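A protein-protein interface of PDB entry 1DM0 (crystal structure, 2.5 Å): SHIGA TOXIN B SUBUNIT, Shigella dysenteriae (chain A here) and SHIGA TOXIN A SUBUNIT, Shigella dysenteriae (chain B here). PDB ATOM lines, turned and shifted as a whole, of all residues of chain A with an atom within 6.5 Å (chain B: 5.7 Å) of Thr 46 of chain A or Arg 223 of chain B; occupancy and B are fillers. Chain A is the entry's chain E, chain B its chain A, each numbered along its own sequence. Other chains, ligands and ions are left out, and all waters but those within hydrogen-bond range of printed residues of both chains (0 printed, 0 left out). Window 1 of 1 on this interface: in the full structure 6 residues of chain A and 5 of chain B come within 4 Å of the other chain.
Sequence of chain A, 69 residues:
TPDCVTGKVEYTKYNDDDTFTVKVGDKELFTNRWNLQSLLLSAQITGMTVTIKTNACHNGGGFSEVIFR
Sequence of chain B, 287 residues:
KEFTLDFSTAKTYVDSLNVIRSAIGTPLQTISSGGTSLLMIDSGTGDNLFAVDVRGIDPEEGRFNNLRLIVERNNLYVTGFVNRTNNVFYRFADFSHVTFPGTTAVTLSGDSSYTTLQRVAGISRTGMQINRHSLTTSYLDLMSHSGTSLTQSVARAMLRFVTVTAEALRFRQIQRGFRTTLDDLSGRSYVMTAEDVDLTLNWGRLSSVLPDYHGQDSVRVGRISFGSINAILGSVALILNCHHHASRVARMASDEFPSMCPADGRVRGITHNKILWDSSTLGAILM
Of the 12 printed residues of chain A, 6 touch a printed residue of chain B.
Hydrophobic or aromatic side chains of chain A within 4 Å of the printed part of chain B: Ile 45.
Among the printed residues, pairs that only touch across the chains: Ile 45 of chain A with Gly 222 of chain B, Thr 46 of chain A with Gly 222 of chain B, Gly 47 of chain A with Arg 223 of chain B, Thr 46 of chain A with Arg 223 of chain B, Thr 46 of chain A with Ile 285 of chain B and Ile 45 of chain A with Thr 281 of chain B.
The backbone carbonyl oxygen (O) of Ser 42 of chain A lies within hydrogen-bond range of the side-chain hydroxyl (OG1) of Thr 46 of chain A (3.1 Å).
The guanidinium group (NH1) of Arg 223 of chain B lies within salt-bridge range of the side-chain carboxylate (OD2) of Asp 198 of chain B, at 3.7 Å.
The side-chain hydroxyl (OG1) of Thr 281 of chain B is in hydrogen-bond range of the backbone NH (N) of Gly 222 of chain B.
Of chain B, only Gly 222, Arg 223 and Ile 285 come within 4 Å of Thr 46 of chain A.
Arg 223 of chain B touches just these residues of chain A: Val 9, Gln 44, Ile 45, Thr 46 and Gly 47.
Printed residues of chain B within 4 Å of Gly 47 of chain A: Arg 223.
Of the printed residues of chain B, Lys 8 of chain A touches Glu 195.
Printed residues of chain B within 4 Å of Ile 45 of chain A: Gly 222, Arg 223 and Thr 281.
Of the printed residues of chain A, Glu 195 of chain B touches Lys 8.
Of the printed residues of chain B, Gln 44 of chain A touches Arg 223 (3.2 Å).
Ser 225 of chain B touches none of the printed residues of chain A.
Val 221 of chain B touches none of the printed residues of chain A.
The nearest residue of chain B that does not touch Thr 46 of chain A is Thr 281 of chain B (4.2 Å).
The nearest printed residue of chain B that does not touch Lys 8 of chain A is Arg 223 of chain B (4.1 Å).
NE of Arg 223 of chain B sits at hydrogen-bond distance from O of Gln 44 of chain A (3.2 Å).
The backbone NH (N) of Arg 223 of chain B lies within hydrogen-bond range of the backbone carbonyl oxygen (O) of Ile 45 of chain A (3.4 Å).
The side-chain amino group of Lys 8 of chain A is in salt-bridge range of the side-chain carboxylate of Glu 195 of chain B (3.1 Å).
The backbone carbonyl oxygen (O) of Val 9 of chain A sits close to the guanidinium group (NH2) of Arg 223 of chain B, at 2.3 Å.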
ATOM      1  N   LYS A   8     -22.341  15.660 -11.683  1.00  0.00           N
ATOM      2  CA  LYS A   8     -21.304  15.575 -12.659  1.00  0.00           C
ATOM      3  C   LYS A   8     -20.333  16.731 -12.481  1.00  0.00           C
ATOM      4  O   LYS A   8     -20.680  17.703 -11.876  1.00  0.00           O
ATOM      5  CB  LYS A   8     -21.819  15.540 -14.110  1.00  0.00           C
ATOM      6  CG  LYS A   8     -23.135  14.911 -14.391  1.00  0.00           C
ATOM      7  CD  LYS A   8     -23.422  14.735 -15.915  1.00  0.00           C
ATOM      8  CE  LYS A   8     -24.919  14.353 -16.192  1.00  0.00           C
ATOM      9  NZ  LYS A   8     -25.138  14.281 -17.647  1.00  0.00           N
ATOM     10  N   VAL A   9     -19.155  16.667 -13.100  1.00  0.00           N
ATOM     11  CA  VAL A   9     -18.146  17.713 -12.982  1.00  0.00           C
ATOM     12  C   VAL A   9     -18.376  18.744 -14.107  1.00  0.00           C
ATOM     13  O   VAL A   9     -18.517  18.356 -15.269  1.00  0.00           O
ATOM     14  CB  VAL A   9     -16.747  17.002 -13.090  1.00  0.00           C
ATOM     15  CG1 VAL A   9     -15.631  17.975 -13.364  1.00  0.00           C
ATOM     16  CG2 VAL A   9     -16.432  16.027 -11.825  1.00  0.00           C
ATOM     17  N   GLU A  10     -18.391  20.047 -13.814  1.00  0.00           N
ATOM     18  CA  GLU A  10     -18.678  21.017 -14.866  1.00  0.00           C
ATOM     19  C   GLU A  10     -17.460  21.493 -15.539  1.00  0.00           C
ATOM     20  O   GLU A  10     -17.415  21.620 -16.733  1.00  0.00           O
ATOM     21  CB  GLU A  10     -19.295  22.234 -14.304  1.00  0.00           C
ATOM     22  CG  GLU A  10     -20.647  21.986 -13.761  1.00  0.00           C
ATOM     23  CD  GLU A  10     -21.330  23.315 -13.423  1.00  0.00           C
ATOM     24  OE1 GLU A  10     -20.924  24.396 -14.028  1.00  0.00           O
ATOM     25  OE2 GLU A  10     -22.242  23.270 -12.527  1.00  0.00           O
ATOM     26  N   TYR A  11     -16.447  21.824 -14.769  1.00  0.00           N
ATOM     27  CA  TYR A  11     -15.166  22.126 -15.335  1.00  0.00           C
ATOM     28  C   TYR A  11     -14.234  21.775 -14.204  1.00  0.00           C
ATOM     29  O   TYR A  11     -14.673  21.527 -13.069  1.00  0.00           O
ATOM     30  CB  TYR A  11     -15.046  23.567 -15.712  1.00  0.00           C
ATOM     31  CG  TYR A  11     -15.216  24.520 -14.569  1.00  0.00           C
ATOM     32  CD1 TYR A  11     -14.153  24.891 -13.765  1.00  0.00           C
ATOM     33  CD2 TYR A  11     -16.457  25.122 -14.329  1.00  0.00           C
ATOM     34  CE1 TYR A  11     -14.366  25.746 -12.666  1.00  0.00           C
ATOM     35  CE2 TYR A  11     -16.667  26.006 -13.276  1.00  0.00           C
ATOM     36  CZ  TYR A  11     -15.652  26.287 -12.449  1.00  0.00           C
ATOM     37  OH  TYR A  11     -15.931  27.198 -11.491  1.00  0.00           O
ATOM     38  N   LEU A  41     -10.351  14.555 -14.172  1.00  0.00           N
ATOM     39  CA  LEU A  41     -10.356  14.902 -15.603  1.00  0.00           C
ATOM     40  C   LEU A  41     -11.107  13.947 -16.506  1.00  0.00           C
ATOM     41  O   LEU A  41     -11.755  14.418 -17.406  1.00  0.00           O
ATOM     42  CB  LEU A  41      -9.074  15.440 -16.262  1.00  0.00           C
ATOM     43  CG  LEU A  41      -9.407  15.916 -17.679  1.00  0.00           C
ATOM     44  CD1 LEU A  41     -10.174  17.176 -17.635  1.00  0.00           C
ATOM     45  CD2 LEU A  41      -8.281  16.052 -18.600  1.00  0.00           C
ATOM     46  N   SER A  42     -11.186  12.662 -16.135  1.00  0.00           N
ATOM     47  CA  SER A  42     -11.888  11.608 -16.910  1.00  0.00           C
ATOM     48  C   SER A  42     -13.393  11.524 -16.561  1.00  0.00           C
ATOM     49  O   SER A  42     -14.215  11.178 -17.392  1.00  0.00           O
ATOM     50  CB  SER A  42     -11.220  10.246 -16.631  1.00  0.00           C
ATOM     51  OG  SER A  42      -9.795  10.296 -16.774  1.00  0.00           O
ATOM     52  N   ALA A  43     -13.731  11.761 -15.306  1.00  0.00           N
ATOM     53  CA  ALA A  43     -15.099  11.853 -14.886  1.00  0.00           C
ATOM     54  C   ALA A  43     -15.675  12.972 -15.681  1.00  0.00           C
ATOM     55  O   ALA A  43     -16.836  12.964 -16.042  1.00  0.00           O
ATOM     56  CB  ALA A  43     -15.165  12.240 -13.479  1.00  0.00           C
ATOM     57  N   GLN A  44     -14.920  14.040 -15.864  1.00  0.00           N
ATOM     58  CA  GLN A  44     -15.515  15.127 -16.601  1.00  0.00           C
ATOM     59  C   GLN A  44     -15.759  14.679 -18.041  1.00  0.00           C
ATOM     60  O   GLN A  44     -16.872  14.819 -18.546  1.00  0.00           O
ATOM     61  CB  GLN A  44     -14.663  16.364 -16.503  1.00  0.00           C
ATOM     62  CG  GLN A  44     -15.012  17.435 -17.505  1.00  0.00           C
ATOM     63  CD  GLN A  44     -14.233  18.676 -17.259  1.00  0.00           C
ATOM     64  OE1 GLN A  44     -13.743  18.857 -16.193  1.00  0.00           O
ATOM     65  NE2 GLN A  44     -14.124  19.542 -18.237  1.00  0.00           N
ATOM     66  N   ILE A  45     -14.753  14.059 -18.675  1.00  0.00           N
ATOM     67  CA  ILE A  45     -14.859  13.637 -20.077  1.00  0.00           C
ATOM     68  C   ILE A  45     -15.974  12.648 -20.370  1.00  0.00           C
ATOM     69  O   ILE A  45     -16.433  12.561 -21.484  1.00  0.00           O
ATOM     70  CB  ILE A  45     -13.552  13.065 -20.582  1.00  0.00           C
ATOM     71  CG1 ILE A  45     -12.548  14.150 -20.872  1.00  0.00           C
ATOM     72  CG2 ILE A  45     -13.718  12.214 -21.834  1.00  0.00           C
ATOM     73  CD1 ILE A  45     -11.121  13.610 -20.815  1.00  0.00           C
ATOM     74  N   THR A  46     -16.434  11.900 -19.392  1.00  0.00           N
ATOM     75  CA  THR A  46     -17.467  10.898 -19.697  1.00  0.00           C
ATOM     76  C   THR A  46     -18.833  11.165 -18.995  1.00  0.00           C
ATOM     77  O   THR A  46     -19.691  10.289 -18.935  1.00  0.00           O
ATOM     78  CB  THR A  46     -16.992   9.447 -19.306  1.00  0.00           C
ATOM     79  OG1 THR A  46     -16.710   9.433 -17.933  1.00  0.00           O
ATOM     80  CG2 THR A  46     -15.704   9.040 -20.003  1.00  0.00           C
ATOM     81  N   GLY A  47     -19.046  12.359 -18.470  1.00  0.00           N
ATOM     82  CA  GLY A  47     -20.302  12.648 -17.832  1.00  0.00           C
ATOM     83  C   GLY A  47     -20.623  11.862 -16.589  1.00  0.00           C
ATOM     84  O   GLY A  47     -21.772  11.801 -16.269  1.00  0.00           O
ATOM     85  N   MET A  48     -19.641  11.362 -15.831  1.00  0.00           N
ATOM     86  CA  MET A  48     -19.870  10.603 -14.583  1.00  0.00           C
ATOM     87  C   MET A  48     -20.347  11.468 -13.454  1.00  0.00           C
ATOM     88  O   MET A  48     -19.918  12.610 -13.337  1.00  0.00           O
ATOM     89  CB  MET A  48     -18.551   9.990 -14.045  1.00  0.00           C
ATOM     90  CG  MET A  48     -17.995   8.653 -14.651  1.00  0.00           C
ATOM     91  SD  MET A  48     -16.727   8.158 -13.525  1.00  0.00           S
ATOM     92  CE  MET A  48     -17.108   6.450 -13.404  1.00  0.00           C
ATOM     93  N   GLU B 195     -27.547  19.034 -20.007  1.00  0.00           N
ATOM     94  CA  GLU B 195     -27.559  17.747 -20.740  1.00  0.00           C
ATOM     95  C   GLU B 195     -27.887  17.874 -22.203  1.00  0.00           C
ATOM     96  O   GLU B 195     -27.396  17.102 -22.982  1.00  0.00           O
ATOM     97  CB  GLU B 195     -28.409  16.705 -20.071  1.00  0.00           C
ATOM     98  CG  GLU B 195     -27.712  16.026 -18.985  1.00  0.00           C
ATOM     99  CD  GLU B 195     -27.614  16.923 -17.836  1.00  0.00           C
ATOM    100  OE1 GLU B 195     -28.624  17.643 -17.663  1.00  0.00           O
ATOM    101  OE2 GLU B 195     -26.569  16.959 -17.120  1.00  0.00           O
ATOM    102  N   ASP B 198     -24.630  19.368 -24.032  1.00  0.00           N
ATOM    103  CA  ASP B 198     -23.630  18.323 -24.332  1.00  0.00           C
ATOM    104  C   ASP B 198     -23.968  17.646 -25.632  1.00  0.00           C
ATOM    105  O   ASP B 198     -23.073  17.222 -26.361  1.00  0.00           O
ATOM    106  CB  ASP B 198     -23.724  17.147 -23.347  1.00  0.00           C
ATOM    107  CG  ASP B 198     -22.979  17.364 -22.080  1.00  0.00           C
ATOM    108  OD1 ASP B 198     -22.272  18.395 -22.015  1.00  0.00           O
ATOM    109  OD2 ASP B 198     -23.153  16.520 -21.144  1.00  0.00           O
ATOM    110  N   ASN B 202     -22.136  17.039 -29.392  1.00  0.00           N
ATOM    111  CA  ASN B 202     -21.656  15.683 -29.744  1.00  0.00           C
ATOM    112  C   ASN B 202     -22.266  15.090 -31.045  1.00  0.00           C
ATOM    113  O   ASN B 202     -22.134  13.877 -31.317  1.00  0.00           O
ATOM    114  CB  ASN B 202     -21.809  14.677 -28.564  1.00  0.00           C
ATOM    115  CG  ASN B 202     -20.888  14.962 -27.410  1.00  0.00           C
ATOM    116  OD1 ASN B 202     -19.698  14.646 -27.494  1.00  0.00           O
ATOM    117  ND2 ASN B 202     -21.422  15.515 -26.291  1.00  0.00           N
ATOM    118  N   VAL B 221     -20.571   8.154 -26.202  1.00  0.00           N
ATOM    119  CA  VAL B 221     -19.716   9.035 -26.931  1.00  0.00           C
ATOM    120  C   VAL B 221     -19.542  10.192 -26.003  1.00  0.00           C
ATOM    121  O   VAL B 221     -20.513  10.837 -25.580  1.00  0.00           O
ATOM    122  CB  VAL B 221     -20.381   9.533 -28.182  1.00  0.00           C
ATOM    123  CG1 VAL B 221     -19.356  10.295 -29.080  1.00  0.00           C
ATOM    124  CG2 VAL B 221     -20.973   8.385 -28.886  1.00  0.00           C
ATOM    125  N   GLY B 222     -18.294  10.413 -25.614  1.00  0.00           N
ATOM    126  CA  GLY B 222     -17.975  11.501 -24.721  1.00  0.00           C
ATOM    127  C   GLY B 222     -18.802  11.489 -23.480  1.00  0.00           C
ATOM    128  O   GLY B 222     -19.037  10.454 -22.835  1.00  0.00           O
ATOM    129  N   ARG B 223     -19.339  12.650 -23.209  1.00  0.00           N
ATOM    130  CA  ARG B 223     -20.091  12.900 -22.000  1.00  0.00           C
ATOM    131  C   ARG B 223     -21.543  12.454 -22.083  1.00  0.00           C
ATOM    132  O   ARG B 223     -22.299  12.655 -21.117  1.00  0.00           O
ATOM    133  CB  ARG B 223     -19.951  14.373 -21.746  1.00  0.00           C
ATOM    134  CG  ARG B 223     -20.542  14.897 -20.586  1.00  0.00           C
ATOM    135  CD  ARG B 223     -20.138  16.335 -20.480  1.00  0.00           C
ATOM    136  NE  ARG B 223     -19.456  16.513 -19.241  1.00  0.00           N
ATOM    137  CZ  ARG B 223     -19.997  16.965 -18.137  1.00  0.00           C
ATOM    138  NH1 ARG B 223     -21.218  17.427 -18.103  1.00  0.00           N
ATOM    139  NH2 ARG B 223     -19.215  17.170 -17.119  1.00  0.00           N
ATOM    140  N   ILE B 224     -21.860  11.679 -23.141  1.00  0.00           N
ATOM    141  CA  ILE B 224     -23.202  11.103 -23.424  1.00  0.00           C
ATOM    142  C   ILE B 224     -23.291   9.566 -23.429  1.00  0.00           C
ATOM    143  O   ILE B 224     -22.529   8.909 -24.113  1.00  0.00           O
ATOM    144  CB  ILE B 224     -23.705  11.571 -24.804  1.00  0.00           C
ATOM    145  CG1 ILE B 224     -24.213  12.974 -24.758  1.00  0.00           C
ATOM    146  CG2 ILE B 224     -24.748  10.686 -25.385  1.00  0.00           C
ATOM    147  CD1 ILE B 224     -23.575  13.634 -25.860  1.00  0.00           C
ATOM    148  N   SER B 225     -24.286   8.988 -22.771  1.00  0.00           N
ATOM    149  CA  SER B 225     -24.420   7.550 -22.815  1.00  0.00           C
ATOM    150  C   SER B 225     -25.884   7.182 -23.092  1.00  0.00           C
ATOM    151  O   SER B 225     -26.800   7.859 -22.618  1.00  0.00           O
ATOM    152  CB  SER B 225     -24.205   7.025 -21.463  1.00  0.00           C
ATOM    153  OG  SER B 225     -25.537   6.934 -21.008  1.00  0.00           O
ATOM    154  N   TRP B 277     -18.135   2.301 -28.081  1.00  0.00           N
ATOM    155  CA  TRP B 277     -17.463   3.539 -27.683  1.00  0.00           C
ATOM    156  C   TRP B 277     -16.957   4.302 -28.900  1.00  0.00           C
ATOM    157  O   TRP B 277     -16.912   3.748 -29.982  1.00  0.00           O
ATOM    158  CB  TRP B 277     -16.234   3.177 -26.892  1.00  0.00           C
ATOM    159  CG  TRP B 277     -16.474   2.857 -25.462  1.00  0.00           C
ATOM    160  CD1 TRP B 277     -16.571   1.611 -24.897  1.00  0.00           C
ATOM    161  CD2 TRP B 277     -16.576   3.798 -24.377  1.00  0.00           C
ATOM    162  NE1 TRP B 277     -16.776   1.735 -23.539  1.00  0.00           N
ATOM    163  CE2 TRP B 277     -16.723   3.060 -23.196  1.00  0.00           C
ATOM    164  CE3 TRP B 277     -16.633   5.186 -24.304  1.00  0.00           C
ATOM    165  CZ2 TRP B 277     -16.911   3.666 -21.967  1.00  0.00           C
ATOM    166  CZ3 TRP B 277     -16.788   5.792 -23.053  1.00  0.00           C
ATOM    167  CH2 TRP B 277     -16.974   5.037 -21.927  1.00  0.00           C
ATOM    168  N   THR B 281     -12.714   8.936 -27.233  1.00  0.00           N
ATOM    169  CA  THR B 281     -12.965   9.067 -25.819  1.00  0.00           C
ATOM    170  C   THR B 281     -12.262   7.961 -25.039  1.00  0.00           C
ATOM    171  O   THR B 281     -11.792   8.190 -23.955  1.00  0.00           O
ATOM    172  CB  THR B 281     -14.454   9.033 -25.511  1.00  0.00           C
ATOM    173  OG1 THR B 281     -15.037  10.223 -26.035  1.00  0.00           O
ATOM    174  CG2 THR B 281     -14.656   9.045 -24.048  1.00  0.00           C
ATOM    175  N   ILE B 285      -9.236   8.432 -22.042  1.00  0.00           N
ATOM    176  CA  ILE B 285      -9.429   8.054 -20.638  1.00  0.00           C
ATOM    177  C   ILE B 285      -8.485   6.897 -20.191  1.00  0.00           C
ATOM    178  O   ILE B 285      -8.536   6.438 -19.044  1.00  0.00           O
ATOM    179  CB  ILE B 285     -10.925   7.657 -20.310  1.00  0.00           C
ATOM    180  CG1 ILE B 285     -11.311   6.326 -20.919  1.00  0.00           C
ATOM    181  CG2 ILE B 285     -11.885   8.590 -20.857  1.00  0.00           C
ATOM    182  CD1 ILE B 285     -12.732   5.974 -20.683  1.00  0.00           C
